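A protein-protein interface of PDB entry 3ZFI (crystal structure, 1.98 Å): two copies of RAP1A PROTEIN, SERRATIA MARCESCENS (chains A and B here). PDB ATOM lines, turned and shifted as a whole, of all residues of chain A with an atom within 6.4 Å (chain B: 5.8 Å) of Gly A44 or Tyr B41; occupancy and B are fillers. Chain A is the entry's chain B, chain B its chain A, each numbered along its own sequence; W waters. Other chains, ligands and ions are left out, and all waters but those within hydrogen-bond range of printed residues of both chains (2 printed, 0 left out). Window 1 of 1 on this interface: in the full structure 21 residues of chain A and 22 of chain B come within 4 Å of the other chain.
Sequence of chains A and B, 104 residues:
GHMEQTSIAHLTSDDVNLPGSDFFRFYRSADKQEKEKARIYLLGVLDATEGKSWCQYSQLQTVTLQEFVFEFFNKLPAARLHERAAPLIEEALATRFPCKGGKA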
ATOM      1  N   ARG A  39      29.980   2.126 -23.218  1.00  0.00           N
ATOM      2  CA  ARG A  39      28.960   3.019 -23.724  1.00  0.00           C
ATOM      3  C   ARG A  39      27.635   2.311 -23.963  1.00  0.00           C
ATOM      4  O   ARG A  39      26.548   2.961 -23.921  1.00  0.00           O
ATOM      5  CB  ARG A  39      29.385   3.606 -25.102  1.00  0.00           C
ATOM      6  CG  ARG A  39      30.414   4.691 -25.064  1.00  0.00           C
ATOM      7  CD  ARG A  39      30.728   4.688 -26.521  1.00  0.00           C
ATOM      8  NE  ARG A  39      31.808   5.469 -26.917  1.00  0.00           N
ATOM      9  CZ  ARG A  39      32.533   5.195 -28.000  1.00  0.00           C
ATOM     10  NH1 ARG A  39      32.329   4.101 -28.774  1.00  0.00           N
ATOM     11  NH2 ARG A  39      33.468   6.047 -28.268  1.00  0.00           N
ATOM     12  N   ILE A  40      27.684   1.039 -24.296  1.00  0.00           N
ATOM     13  CA  ILE A  40      26.432   0.284 -24.398  1.00  0.00           C
ATOM     14  C   ILE A  40      25.802   0.027 -23.005  1.00  0.00           C
ATOM     15  O   ILE A  40      24.614   0.052 -22.860  1.00  0.00           O
ATOM     16  CB  ILE A  40      26.630  -1.030 -25.211  1.00  0.00           C
ATOM     17  CG1 ILE A  40      26.919  -0.737 -26.723  1.00  0.00           C
ATOM     18  CG2 ILE A  40      25.451  -1.965 -25.023  1.00  0.00           C
ATOM     19  CD1 ILE A  40      27.458  -1.968 -27.465  1.00  0.00           C
ATOM     20  N   TYR A  41      26.616  -0.256 -22.025  1.00  0.00           N
ATOM     21  CA  TYR A  41      26.167  -0.239 -20.627  1.00  0.00           C
ATOM     22  C   TYR A  41      25.464   1.057 -20.252  1.00  0.00           C
ATOM     23  O   TYR A  41      24.330   1.013 -19.690  1.00  0.00           O
ATOM     24  CB  TYR A  41      27.344  -0.477 -19.650  1.00  0.00           C
ATOM     25  CG  TYR A  41      26.913  -0.398 -18.140  1.00  0.00           C
ATOM     26  CD1 TYR A  41      26.976   0.829 -17.433  1.00  0.00           C
ATOM     27  CD2 TYR A  41      26.521  -1.553 -17.433  1.00  0.00           C
ATOM     28  CE1 TYR A  41      26.621   0.912 -16.071  1.00  0.00           C
ATOM     29  CE2 TYR A  41      26.144  -1.489 -16.049  1.00  0.00           C
ATOM     30  CZ  TYR A  41      26.215  -0.238 -15.382  1.00  0.00           C
ATOM     31  OH  TYR A  41      25.900  -0.096 -14.025  1.00  0.00           O
ATOM     32  N   LEU A  42      26.085   2.181 -20.609  1.00  0.00           N
ATOM     33  CA  LEU A  42      25.517   3.531 -20.374  1.00  0.00           C
ATOM     34  C   LEU A  42      24.165   3.716 -21.131  1.00  0.00           C
ATOM     35  O   LEU A  42      23.162   4.169 -20.561  1.00  0.00           O
ATOM     36  CB  LEU A  42      26.510   4.584 -20.809  1.00  0.00           C
ATOM     37  CG  LEU A  42      26.014   6.039 -20.881  1.00  0.00           C
ATOM     38  CD1 LEU A  42      25.507   6.509 -19.513  1.00  0.00           C
ATOM     39  CD2 LEU A  42      27.091   6.985 -21.390  1.00  0.00           C
ATOM     40  N   LEU A  43      24.126   3.222 -22.356  1.00  0.00           N
ATOM     41  CA  LEU A  43      22.876   3.163 -23.131  1.00  0.00           C
ATOM     42  C   LEU A  43      21.751   2.407 -22.394  1.00  0.00           C
ATOM     43  O   LEU A  43      20.592   2.869 -22.387  1.00  0.00           O
ATOM     44  CB  LEU A  43      23.133   2.628 -24.573  1.00  0.00           C
ATOM     45  CG  LEU A  43      21.839   2.339 -25.348  1.00  0.00           C
ATOM     46  CD1 LEU A  43      21.220   3.682 -25.711  1.00  0.00           C
ATOM     47  CD2 LEU A  43      22.222   1.560 -26.599  1.00  0.00           C
ATOM     48  N   GLY A  44      22.041   1.224 -21.827  1.00  0.00           N
ATOM     49  CA  GLY A  44      20.947   0.527 -21.053  1.00  0.00           C
ATOM     50  C   GLY A  44      20.543   1.431 -19.875  1.00  0.00           C
ATOM     51  O   GLY A  44      19.355   1.550 -19.589  1.00  0.00           O
ATOM     52  N   VAL A  45      21.504   2.045 -19.171  1.00  0.00           N
ATOM     53  CA  VAL A  45      21.163   2.961 -18.035  1.00  0.00           C
ATOM     54  C   VAL A  45      20.286   4.173 -18.501  1.00  0.00           C
ATOM     55  O   VAL A  45      19.232   4.499 -17.897  1.00  0.00           O
ATOM     56  CB  VAL A  45      22.415   3.472 -17.266  1.00  0.00           C
ATOM     57  CG1 VAL A  45      22.018   4.476 -16.167  1.00  0.00           C
ATOM     58  CG2 VAL A  45      23.197   2.318 -16.678  1.00  0.00           C
ATOM     59  N   LEU A  46      20.702   4.831 -19.566  1.00  0.00           N
ATOM     60  CA  LEU A  46      19.945   5.955 -20.073  1.00  0.00           C
ATOM     61  C   LEU A  46      18.546   5.530 -20.461  1.00  0.00           C
ATOM     62  O   LEU A  46      17.580   6.275 -20.195  1.00  0.00           O
ATOM     63  CB  LEU A  46      20.557   6.549 -21.376  1.00  0.00           C
ATOM     64  CG  LEU A  46      22.004   7.083 -21.197  1.00  0.00           C
ATOM     65  CD1 LEU A  46      22.699   7.182 -22.578  1.00  0.00           C
ATOM     66  CD2 LEU A  46      21.963   8.379 -20.445  1.00  0.00           C
ATOM     67  N   ASP A  47      18.428   4.417 -21.166  1.00  0.00           N
ATOM     68  CA  ASP A  47      17.141   4.066 -21.740  1.00  0.00           C
ATOM     69  C   ASP A  47      16.198   3.740 -20.604  1.00  0.00           C
ATOM     70  O   ASP A  47      14.981   3.962 -20.736  1.00  0.00           O
ATOM     71  CB  ASP A  47      17.239   2.832 -22.652  1.00  0.00           C
ATOM     72  CG  ASP A  47      17.434   3.179 -24.126  1.00  0.00           C
ATOM     73  OD1 ASP A  47      17.623   4.375 -24.448  1.00  0.00           O
ATOM     74  OD2 ASP A  47      17.337   2.240 -24.990  1.00  0.00           O
ATOM     75  N   ALA A  48      16.758   3.178 -19.522  1.00  0.00           N
ATOM     76  CA  ALA A  48      15.999   2.734 -18.334  1.00  0.00           C
ATOM     77  C   ALA A  48      15.471   3.896 -17.452  1.00  0.00           C
ATOM     78  O   ALA A  48      14.554   3.714 -16.659  1.00  0.00           O
ATOM     79  CB  ALA A  48      16.832   1.771 -17.480  1.00  0.00           C
ATOM     80  N   THR A  49      16.061   5.071 -17.594  1.00  0.00           N
ATOM     81  CA  THR A  49      15.792   6.161 -16.667  1.00  0.00           C
ATOM     82  C   THR A  49      15.275   7.387 -17.381  1.00  0.00           C
ATOM     83  O   THR A  49      14.753   8.318 -16.771  1.00  0.00           O
ATOM     84  CB  THR A  49      17.092   6.533 -15.899  1.00  0.00           C
ATOM     85  OG1 THR A  49      18.148   6.784 -16.847  1.00  0.00           O
ATOM     86  CG2 THR A  49      17.552   5.387 -15.064  1.00  0.00           C
ATOM     87  N   LEU B  11      24.076  -3.777 -32.906  1.00  0.00           N
ATOM     88  CA  LEU B  11      23.795  -2.990 -31.726  1.00  0.00           C
ATOM     89  C   LEU B  11      24.989  -2.110 -31.455  1.00  0.00           C
ATOM     90  O   LEU B  11      26.125  -2.598 -31.318  1.00  0.00           O
ATOM     91  CB  LEU B  11      23.455  -3.919 -30.521  1.00  0.00           C
ATOM     92  CG  LEU B  11      23.182  -3.235 -29.189  1.00  0.00           C
ATOM     93  CD1 LEU B  11      22.074  -2.204 -29.335  1.00  0.00           C
ATOM     94  CD2 LEU B  11      22.855  -4.327 -28.167  1.00  0.00           C
ATOM     95  N   ASP B  15      22.398   3.563 -30.296  1.00  0.00           N
ATOM     96  CA  ASP B  15      20.974   3.068 -30.364  1.00  0.00           C
ATOM     97  C   ASP B  15      20.034   3.461 -29.227  1.00  0.00           C
ATOM     98  O   ASP B  15      19.324   2.575 -28.633  1.00  0.00           O
ATOM     99  CB  ASP B  15      20.963   1.540 -30.533  1.00  0.00           C
ATOM    100  CG  ASP B  15      21.542   1.114 -31.856  1.00  0.00           C
ATOM    101  OD1 ASP B  15      21.327   1.830 -32.824  1.00  0.00           O
ATOM    102  OD2 ASP B  15      22.235   0.091 -31.950  1.00  0.00           O
ATOM    103  N   ASN B  17      16.805   4.667 -27.104  1.00  0.00           N
ATOM    104  CA  ASN B  17      15.416   4.181 -27.279  1.00  0.00           C
ATOM    105  C   ASN B  17      15.356   2.940 -28.129  1.00  0.00           C
ATOM    106  O   ASN B  17      14.525   2.841 -29.033  1.00  0.00           O
ATOM    107  CB  ASN B  17      14.526   5.272 -27.901  1.00  0.00           C
ATOM    108  CG  ASN B  17      14.252   6.391 -26.921  1.00  0.00           C
ATOM    109  OD1 ASN B  17      14.390   7.563 -27.260  1.00  0.00           O
ATOM    110  ND2 ASN B  17      13.906   6.031 -25.664  1.00  0.00           N
ATOM    111  N   LEU B  18      16.207   1.965 -27.798  1.00  0.00           N
ATOM    112  CA  LEU B  18      16.270   0.724 -28.547  1.00  0.00           C
ATOM    113  C   LEU B  18      14.887   0.087 -28.471  1.00  0.00           C
ATOM    114  O   LEU B  18      14.359  -0.106 -27.359  1.00  0.00           O
ATOM    115  CB  LEU B  18      17.283  -0.199 -27.881  1.00  0.00           C
ATOM    116  CG  LEU B  18      17.518  -1.565 -28.566  1.00  0.00           C
ATOM    117  CD1 LEU B  18      18.250  -1.358 -29.901  1.00  0.00           C
ATOM    118  CD2 LEU B  18      18.445  -2.317 -27.641  1.00  0.00           C
ATOM    119  N   PHE B  23      16.159  -5.155 -29.787  1.00  0.00           N
ATOM    120  CA  PHE B  23      16.825  -5.775 -28.660  1.00  0.00           C
ATOM    121  C   PHE B  23      16.706  -7.306 -28.795  1.00  0.00           C
ATOM    122  O   PHE B  23      17.694  -8.056 -28.591  1.00  0.00           O
ATOM    123  CB  PHE B  23      16.178  -5.333 -27.338  1.00  0.00           C
ATOM    124  CG  PHE B  23      16.674  -6.133 -26.155  1.00  0.00           C
ATOM    125  CD1 PHE B  23      17.967  -5.920 -25.675  1.00  0.00           C
ATOM    126  CD2 PHE B  23      15.875  -7.154 -25.584  1.00  0.00           C
ATOM    127  CE1 PHE B  23      18.488  -6.702 -24.626  1.00  0.00           C
ATOM    128  CE2 PHE B  23      16.360  -7.935 -24.534  1.00  0.00           C
ATOM    129  CZ  PHE B  23      17.670  -7.711 -24.068  1.00  0.00           C
ATOM    130  N   GLU B  36      26.346 -10.676 -26.821  1.00  0.00           N
ATOM    131  CA  GLU B  36      27.034 -10.211 -25.620  1.00  0.00           C
ATOM    132  C   GLU B  36      26.750  -8.712 -25.458  1.00  0.00           C
ATOM    133  O   GLU B  36      26.433  -8.245 -24.368  1.00  0.00           O
ATOM    134  CB  GLU B  36      28.548 -10.549 -25.663  1.00  0.00           C
ATOM    135  CG  GLU B  36      29.437  -9.828 -24.589  1.00  0.00           C
ATOM    136  CD  GLU B  36      29.110 -10.115 -23.085  1.00  0.00           C
ATOM    137  OE1 GLU B  36      28.149 -10.876 -22.782  1.00  0.00           O
ATOM    138  OE2 GLU B  36      29.801  -9.563 -22.162  1.00  0.00           O
ATOM    139  N   LYS B  37      26.828  -7.943 -26.533  1.00  0.00           N
ATOM    140  CA  LYS B  37      26.426  -6.520 -26.455  1.00  0.00           C
ATOM    141  C   LYS B  37      24.962  -6.320 -25.976  1.00  0.00           C
ATOM    142  O   LYS B  37      24.677  -5.418 -25.237  1.00  0.00           O
ATOM    143  CB  LYS B  37      26.629  -5.805 -27.811  1.00  0.00           C
ATOM    144  CG  LYS B  37      28.105  -5.757 -28.172  1.00  0.00           C
ATOM    145  CD  LYS B  37      28.350  -5.151 -29.543  1.00  0.00           C
ATOM    146  CE  LYS B  37      29.830  -4.817 -29.549  1.00  0.00           C
ATOM    147  NZ  LYS B  37      30.381  -4.217 -30.791  1.00  0.00           N
ATOM    148  N   ALA B  38      24.057  -7.188 -26.403  1.00  0.00           N
ATOM    149  CA  ALA B  38      22.639  -7.105 -26.062  1.00  0.00           C
ATOM    150  C   ALA B  38      22.580  -7.397 -24.582  1.00  0.00           C
ATOM    151  O   ALA B  38      21.828  -6.730 -23.847  1.00  0.00           O
ATOM    152  CB  ALA B  38      21.824  -8.125 -26.843  1.00  0.00           C
ATOM    153  N   ARG B  39      23.408  -8.355 -24.106  1.00  0.00           N
ATOM    154  CA  ARG B  39      23.408  -8.708 -22.674  1.00  0.00           C
ATOM    155  C   ARG B  39      24.025  -7.593 -21.831  1.00  0.00           C
ATOM    156  O   ARG B  39      23.647  -7.398 -20.638  1.00  0.00           O
ATOM    157  CB  ARG B  39      24.006 -10.126 -22.420  1.00  0.00           C
ATOM    158  CG  ARG B  39      22.959 -11.221 -22.669  1.00  0.00           C
ATOM    159  CD  ARG B  39      23.414 -12.642 -23.038  1.00  0.00           C
ATOM    160  NE  ARG B  39      22.203 -13.461 -23.239  1.00  0.00           N
ATOM    161  CZ  ARG B  39      21.536 -13.540 -24.393  1.00  0.00           C
ATOM    162  NH1 ARG B  39      21.964 -12.895 -25.456  1.00  0.00           N
ATOM    163  NH2 ARG B  39      20.430 -14.215 -24.483  1.00  0.00           N
ATOM    164  N   ILE B  40      24.929  -6.844 -22.426  1.00  0.00           N
ATOM    165  CA  ILE B  40      25.504  -5.631 -21.747  1.00  0.00           C
ATOM    166  C   ILE B  40      24.507  -4.449 -21.685  1.00  0.00           C
ATOM    167  O   ILE B  40      24.417  -3.731 -20.680  1.00  0.00           O
ATOM    168  CB  ILE B  40      26.840  -5.192 -22.407  1.00  0.00           C
ATOM    169  CG1 ILE B  40      27.885  -6.340 -22.086  1.00  0.00           C
ATOM    170  CG2 ILE B  40      27.297  -3.841 -21.875  1.00  0.00           C
ATOM    171  CD1 ILE B  40      29.201  -6.167 -22.831  1.00  0.00           C
ATOM    172  N   TYR B  41      23.750  -4.269 -22.763  1.00  0.00           N
ATOM    173  CA  TYR B  41      22.625  -3.310 -22.698  1.00  0.00           C
ATOM    174  C   TYR B  41      21.701  -3.772 -21.536  1.00  0.00           C
ATOM    175  O   TYR B  41      21.363  -2.984 -20.645  1.00  0.00           O
ATOM    176  CB  TYR B  41      21.871  -3.322 -24.019  1.00  0.00           C
ATOM    177  CG  TYR B  41      20.591  -2.474 -24.007  1.00  0.00           C
ATOM    178  CD1 TYR B  41      19.361  -3.019 -23.608  1.00  0.00           C
ATOM    179  CD2 TYR B  41      20.623  -1.099 -24.386  1.00  0.00           C
ATOM    180  CE1 TYR B  41      18.192  -2.244 -23.612  1.00  0.00           C
ATOM    181  CE2 TYR B  41      19.459  -0.333 -24.386  1.00  0.00           C
ATOM    182  CZ  TYR B  41      18.264  -0.922 -23.965  1.00  0.00           C
ATOM    183  OH  TYR B  41      17.106  -0.180 -23.994  1.00  0.00           O
ATOM    184  N   LEU B  42      21.377  -5.078 -21.488  1.00  0.00           N
ATOM    185  CA  LEU B  42      20.567  -5.588 -20.394  1.00  0.00           C
ATOM    186  C   LEU B  42      21.197  -5.320 -19.026  1.00  0.00           C
ATOM    187  O   LEU B  42      20.537  -4.872 -18.090  1.00  0.00           O
ATOM    188  CB  LEU B  42      20.293  -7.070 -20.630  1.00  0.00           C
ATOM    189  CG  LEU B  42      19.692  -7.915 -19.502  1.00  0.00           C
ATOM    190  CD1 LEU B  42      18.277  -7.456 -19.163  1.00  0.00           C
ATOM    191  CD2 LEU B  42      19.715  -9.371 -19.921  1.00  0.00           C
ATOM    192  N   LEU B  43      22.478  -5.618 -18.858  1.00  0.00           N
ATOM    193  CA  LEU B  43      23.158  -5.280 -17.573  1.00  0.00           C
ATOM    194  C   LEU B  43      22.960  -3.780 -17.188  1.00  0.00           C
ATOM    195  O   LEU B  43      22.681  -3.479 -16.051  1.00  0.00           O
ATOM    196  CB  LEU B  43      24.666  -5.515 -17.757  1.00  0.00           C
ATOM    197  CG  LEU B  43      25.591  -5.088 -16.628  1.00  0.00           C
ATOM    198  CD1 LEU B  43      25.196  -5.945 -15.458  1.00  0.00           C
ATOM    199  CD2 LEU B  43      27.056  -5.375 -17.013  1.00  0.00           C
ATOM    200  N   GLY B  44      23.080  -2.847 -18.143  1.00  0.00           N
ATOM    201  CA  GLY B  44      22.854  -1.450 -17.786  1.00  0.00           C
ATOM    202  C   GLY B  44      21.427  -1.242 -17.278  1.00  0.00           C
ATOM    203  O   GLY B  44      21.219  -0.585 -16.266  1.00  0.00           O
ATOM    204  N   VAL B  45      20.454  -1.849 -17.950  1.00  0.00           N
ATOM    205  CA  VAL B  45      19.078  -1.803 -17.454  1.00  0.00           C
ATOM    206  C   VAL B  45      18.865  -2.476 -16.059  1.00  0.00           C
ATOM    207  O   VAL B  45      18.180  -1.884 -15.191  1.00  0.00           O
ATOM    208  CB  VAL B  45      18.125  -2.414 -18.462  1.00  0.00           C
ATOM    209  CG1 VAL B  45      16.713  -2.357 -17.886  1.00  0.00           C
ATOM    210  CG2 VAL B  45      18.230  -1.685 -19.816  1.00  0.00           C
ATOM    211  N   LEU B  46      19.383  -3.696 -15.847  1.00  0.00           N
ATOM    212  CA  LEU B  46      19.342  -4.349 -14.511  1.00  0.00           C
ATOM    213  C   LEU B  46      19.934  -3.437 -13.443  1.00  0.00           C
ATOM    214  O   LEU B  46      19.337  -3.233 -12.365  1.00  0.00           O
ATOM    215  CB  LEU B  46      20.187  -5.640 -14.507  1.00  0.00           C
ATOM    216  CG  LEU B  46      19.861  -6.728 -15.499  1.00  0.00           C
ATOM    217  CD1 LEU B  46      20.896  -7.829 -15.465  1.00  0.00           C
ATOM    218  CD2 LEU B  46      18.421  -7.253 -15.324  1.00  0.00           C
ATOM    219  N   ALA B  48      20.377  -0.287 -13.352  1.00  0.00           N
ATOM    220  CA  ALA B  48      19.689   0.969 -13.130  1.00  0.00           C
ATOM    221  C   ALA B  48      18.376   0.733 -12.365  1.00  0.00           C
ATOM    222  O   ALA B  48      17.853   1.641 -11.737  1.00  0.00           O
ATOM    223  CB  ALA B  48      19.385   1.615 -14.487  1.00  0.00           C
ATOM    224  N   ARG B  84       9.747   0.358 -26.110  1.00  0.00           N
ATOM    225  CA  ARG B  84      11.179   0.485 -25.835  1.00  0.00           C
ATOM    226  C   ARG B  84      11.710  -0.722 -25.040  1.00  0.00           C
ATOM    227  O   ARG B  84      11.058  -1.196 -24.088  1.00  0.00           O
ATOM    228  CB  ARG B  84      11.392   1.771 -25.040  1.00  0.00           C
ATOM    229  CG  ARG B  84      10.944   3.050 -25.782  1.00  0.00           C
ATOM    230  CD  ARG B  84      11.477   4.326 -25.106  1.00  0.00           C
ATOM    231  NE  ARG B  84      11.035   4.394 -23.700  1.00  0.00           N
ATOM    232  CZ  ARG B  84      11.849   4.479 -22.645  1.00  0.00           C
ATOM    233  NH1 ARG B  84      13.180   4.599 -22.836  1.00  0.00           N
ATOM    234  NH2 ARG B  84      11.316   4.499 -21.402  1.00  0.00           N
ATOM    235  N   ALA B  85      12.880  -1.222 -25.410  1.00  0.00           N
ATOM    236  CA  ALA B  85      13.374  -2.422 -24.764  1.00  0.00           C
ATOM    237  C   ALA B  85      13.580  -2.336 -23.228  1.00  0.00           C
ATOM    238  O   ALA B  85      13.310  -3.292 -22.486  1.00  0.00           O
ATOM    239  CB  ALA B  85      14.659  -2.884 -25.445  1.00  0.00           C
ATOM    240  N   ALA B  86      14.101  -1.212 -22.756  1.00  0.00           N
ATOM    241  CA  ALA B  86      14.387  -1.032 -21.336  1.00  0.00           C
ATOM    242  C   ALA B  86      13.146  -1.216 -20.450  1.00  0.00           C
ATOM    243  O   ALA B  86      13.185  -2.061 -19.534  1.00  0.00           O
ATOM    244  CB  ALA B  86      15.111   0.300 -21.056  1.00  0.00           C
ATOM    245  N   ILE B  89      12.092  -4.952 -20.500  1.00  0.00           N
ATOM    246  CA  ILE B  89      12.997  -5.772 -19.639  1.00  0.00           C
ATOM    247  C   ILE B  89      12.618  -5.557 -18.164  1.00  0.00           C
ATOM    248  O   ILE B  89      12.525  -6.504 -17.390  1.00  0.00           O
ATOM    249  CB  ILE B  89      14.466  -5.307 -19.845  1.00  0.00           C
ATOM    250  CG1 ILE B  89      15.015  -5.735 -21.232  1.00  0.00           C
ATOM    251  CG2 ILE B  89      15.335  -5.733 -18.657  1.00  0.00           C
ATOM    252  CD1 ILE B  89      16.338  -5.060 -21.643  1.00  0.00           C
HETATM  253  O   HOH W   1      12.657   5.222 -19.409  1.00  0.00           O
HETATM  254  O   HOH W   2      14.557   1.099 -24.786  1.00  0.00           O
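Of chain B, only Tyr B41 (3.6 Å), Gly B44 (3.8 Å) and Val B45 (3.4 Å) come within 4 Å of Gly A44.
Printed residues of chain A within 4 Å of Tyr B41: Ile A40 (3.6 Å), Leu A43 (3.7 Å), Gly A44 (3.6 Å) and Asp A47 (2.6 Å).
Of the printed residues of chain B, Tyr A41 touches Ile B40, Leu B43 and Gly B44.
Of the printed residues of chain A, Lys B37 touches Ile A40 (3.5 Å).
Of the printed residues of chain B, Val A45 touches Gly B44.
Printed residues of chain A within 4 Å of Leu B43: Tyr A41.
The backbone carbonyl oxygen of Leu B18 lies within hydrogen-bond range of the backbone NH of Ala B85 (2.7 Å).
The side-chain amide nitrogen (ND2) of Asn B17 lies close to the guanidinium group (NH1) of Arg B84 (3.3 Å).
OH of Tyr B41 is in hydrogen-bond range of N of Ala B86 (3.4 Å).
The backbone carbonyl oxygen of Val A45 lies within hydrogen-bond range of the side-chain hydroxyl of Thr A49, 2.7 Å away.
Among the printed residues, pairs that only touch across the chains: Gly A44 with Val B45 (3.4 Å), Tyr A41 with Gly B44 (3.4 Å), Val A45 with Gly B44 (3.5 Å), Ile A40 with Lys B37 (3.5 Å), Gly A44 with Tyr B41 (3.6 Å), Asp A47 with Ala B86 (3.6 Å), Ile A40 with Tyr B41 (3.6 Å), Tyr A41 with Ile B40 (3.7 Å), Ala A48 with Ala B86 (3.7 Å), Leu A43 with Asp B15 (3.7 Å), Tyr A41 with Leu B43 (3.7 Å), Leu A43 with Tyr B41 (3.7 Å), Gly A44 with Gly B44 (3.8 Å) and Ala A48 with Ala B48 (3.9 Å).
Water W1 lies within hydrogen-bond range of NH2 of Arg B84 (2.5 Å) and O of Asp A47 (3.0 Å).
Water W2 lies within hydrogen-bond range of the backbone carbonyl oxygen (O) of Leu B18, the backbone NH (N) of Ala B85, the side-chain hydroxyl (OH) of Tyr B41, the side-chain carboxylate (OD2) of Asp A47 and the backbone NH (N) of Ala B86.
The backbone NH (N) of Leu B18 sits at hydrogen-bond distance from the side-chain carboxylate (OD2) of Asp A47, 3.0 Å away.
The guanidinium group (NH1) of Arg B84 is in hydrogen-bond range of the backbone carbonyl oxygen (O) of Asp A47, 2.8 Å away.
N of Asn B17 lies within hydrogen-bond range of OD1 of Asp A47.
OH of Tyr B41 is in hydrogen-bond range of OD2 of Asp A47, 2.6 Å away.
Printed residues of chain B that touch a printed residue of chain A: Asp B15, Asn B17, Leu B18, Lys B37, Ile B40, Tyr B41, Leu B43, Gly B44, Val B45, Ala B48, Arg B84 and Ala B86.
Printed residues of chain A that touch a printed residue of chain B: Ile A40, Tyr A41, Leu A43, Gly A44, Val A45, Asp A47 and Ala A48.
Hydrophobic or aromatic side chains of chain A within 4 Å of the printed part of chain B: Ile A40, Tyr A41, Leu A43, Val A45 and Ala A48.
Among the printed residues, no Asp or Glu carboxylate lies within 4 Å of a Lys or Arg side-chain nitrogen of the other chain.
Tyr A41 touches Leu B43, and with the chains exchanged Leu A43 touches Tyr B41.
Tyr A41 touches Gly B44, and with the chains exchanged Gly A44 touches Tyr B41.
Gly B44 touches its own counterpart, Gly A44.
Ala B48 touches its own counterpart, Ala A48.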
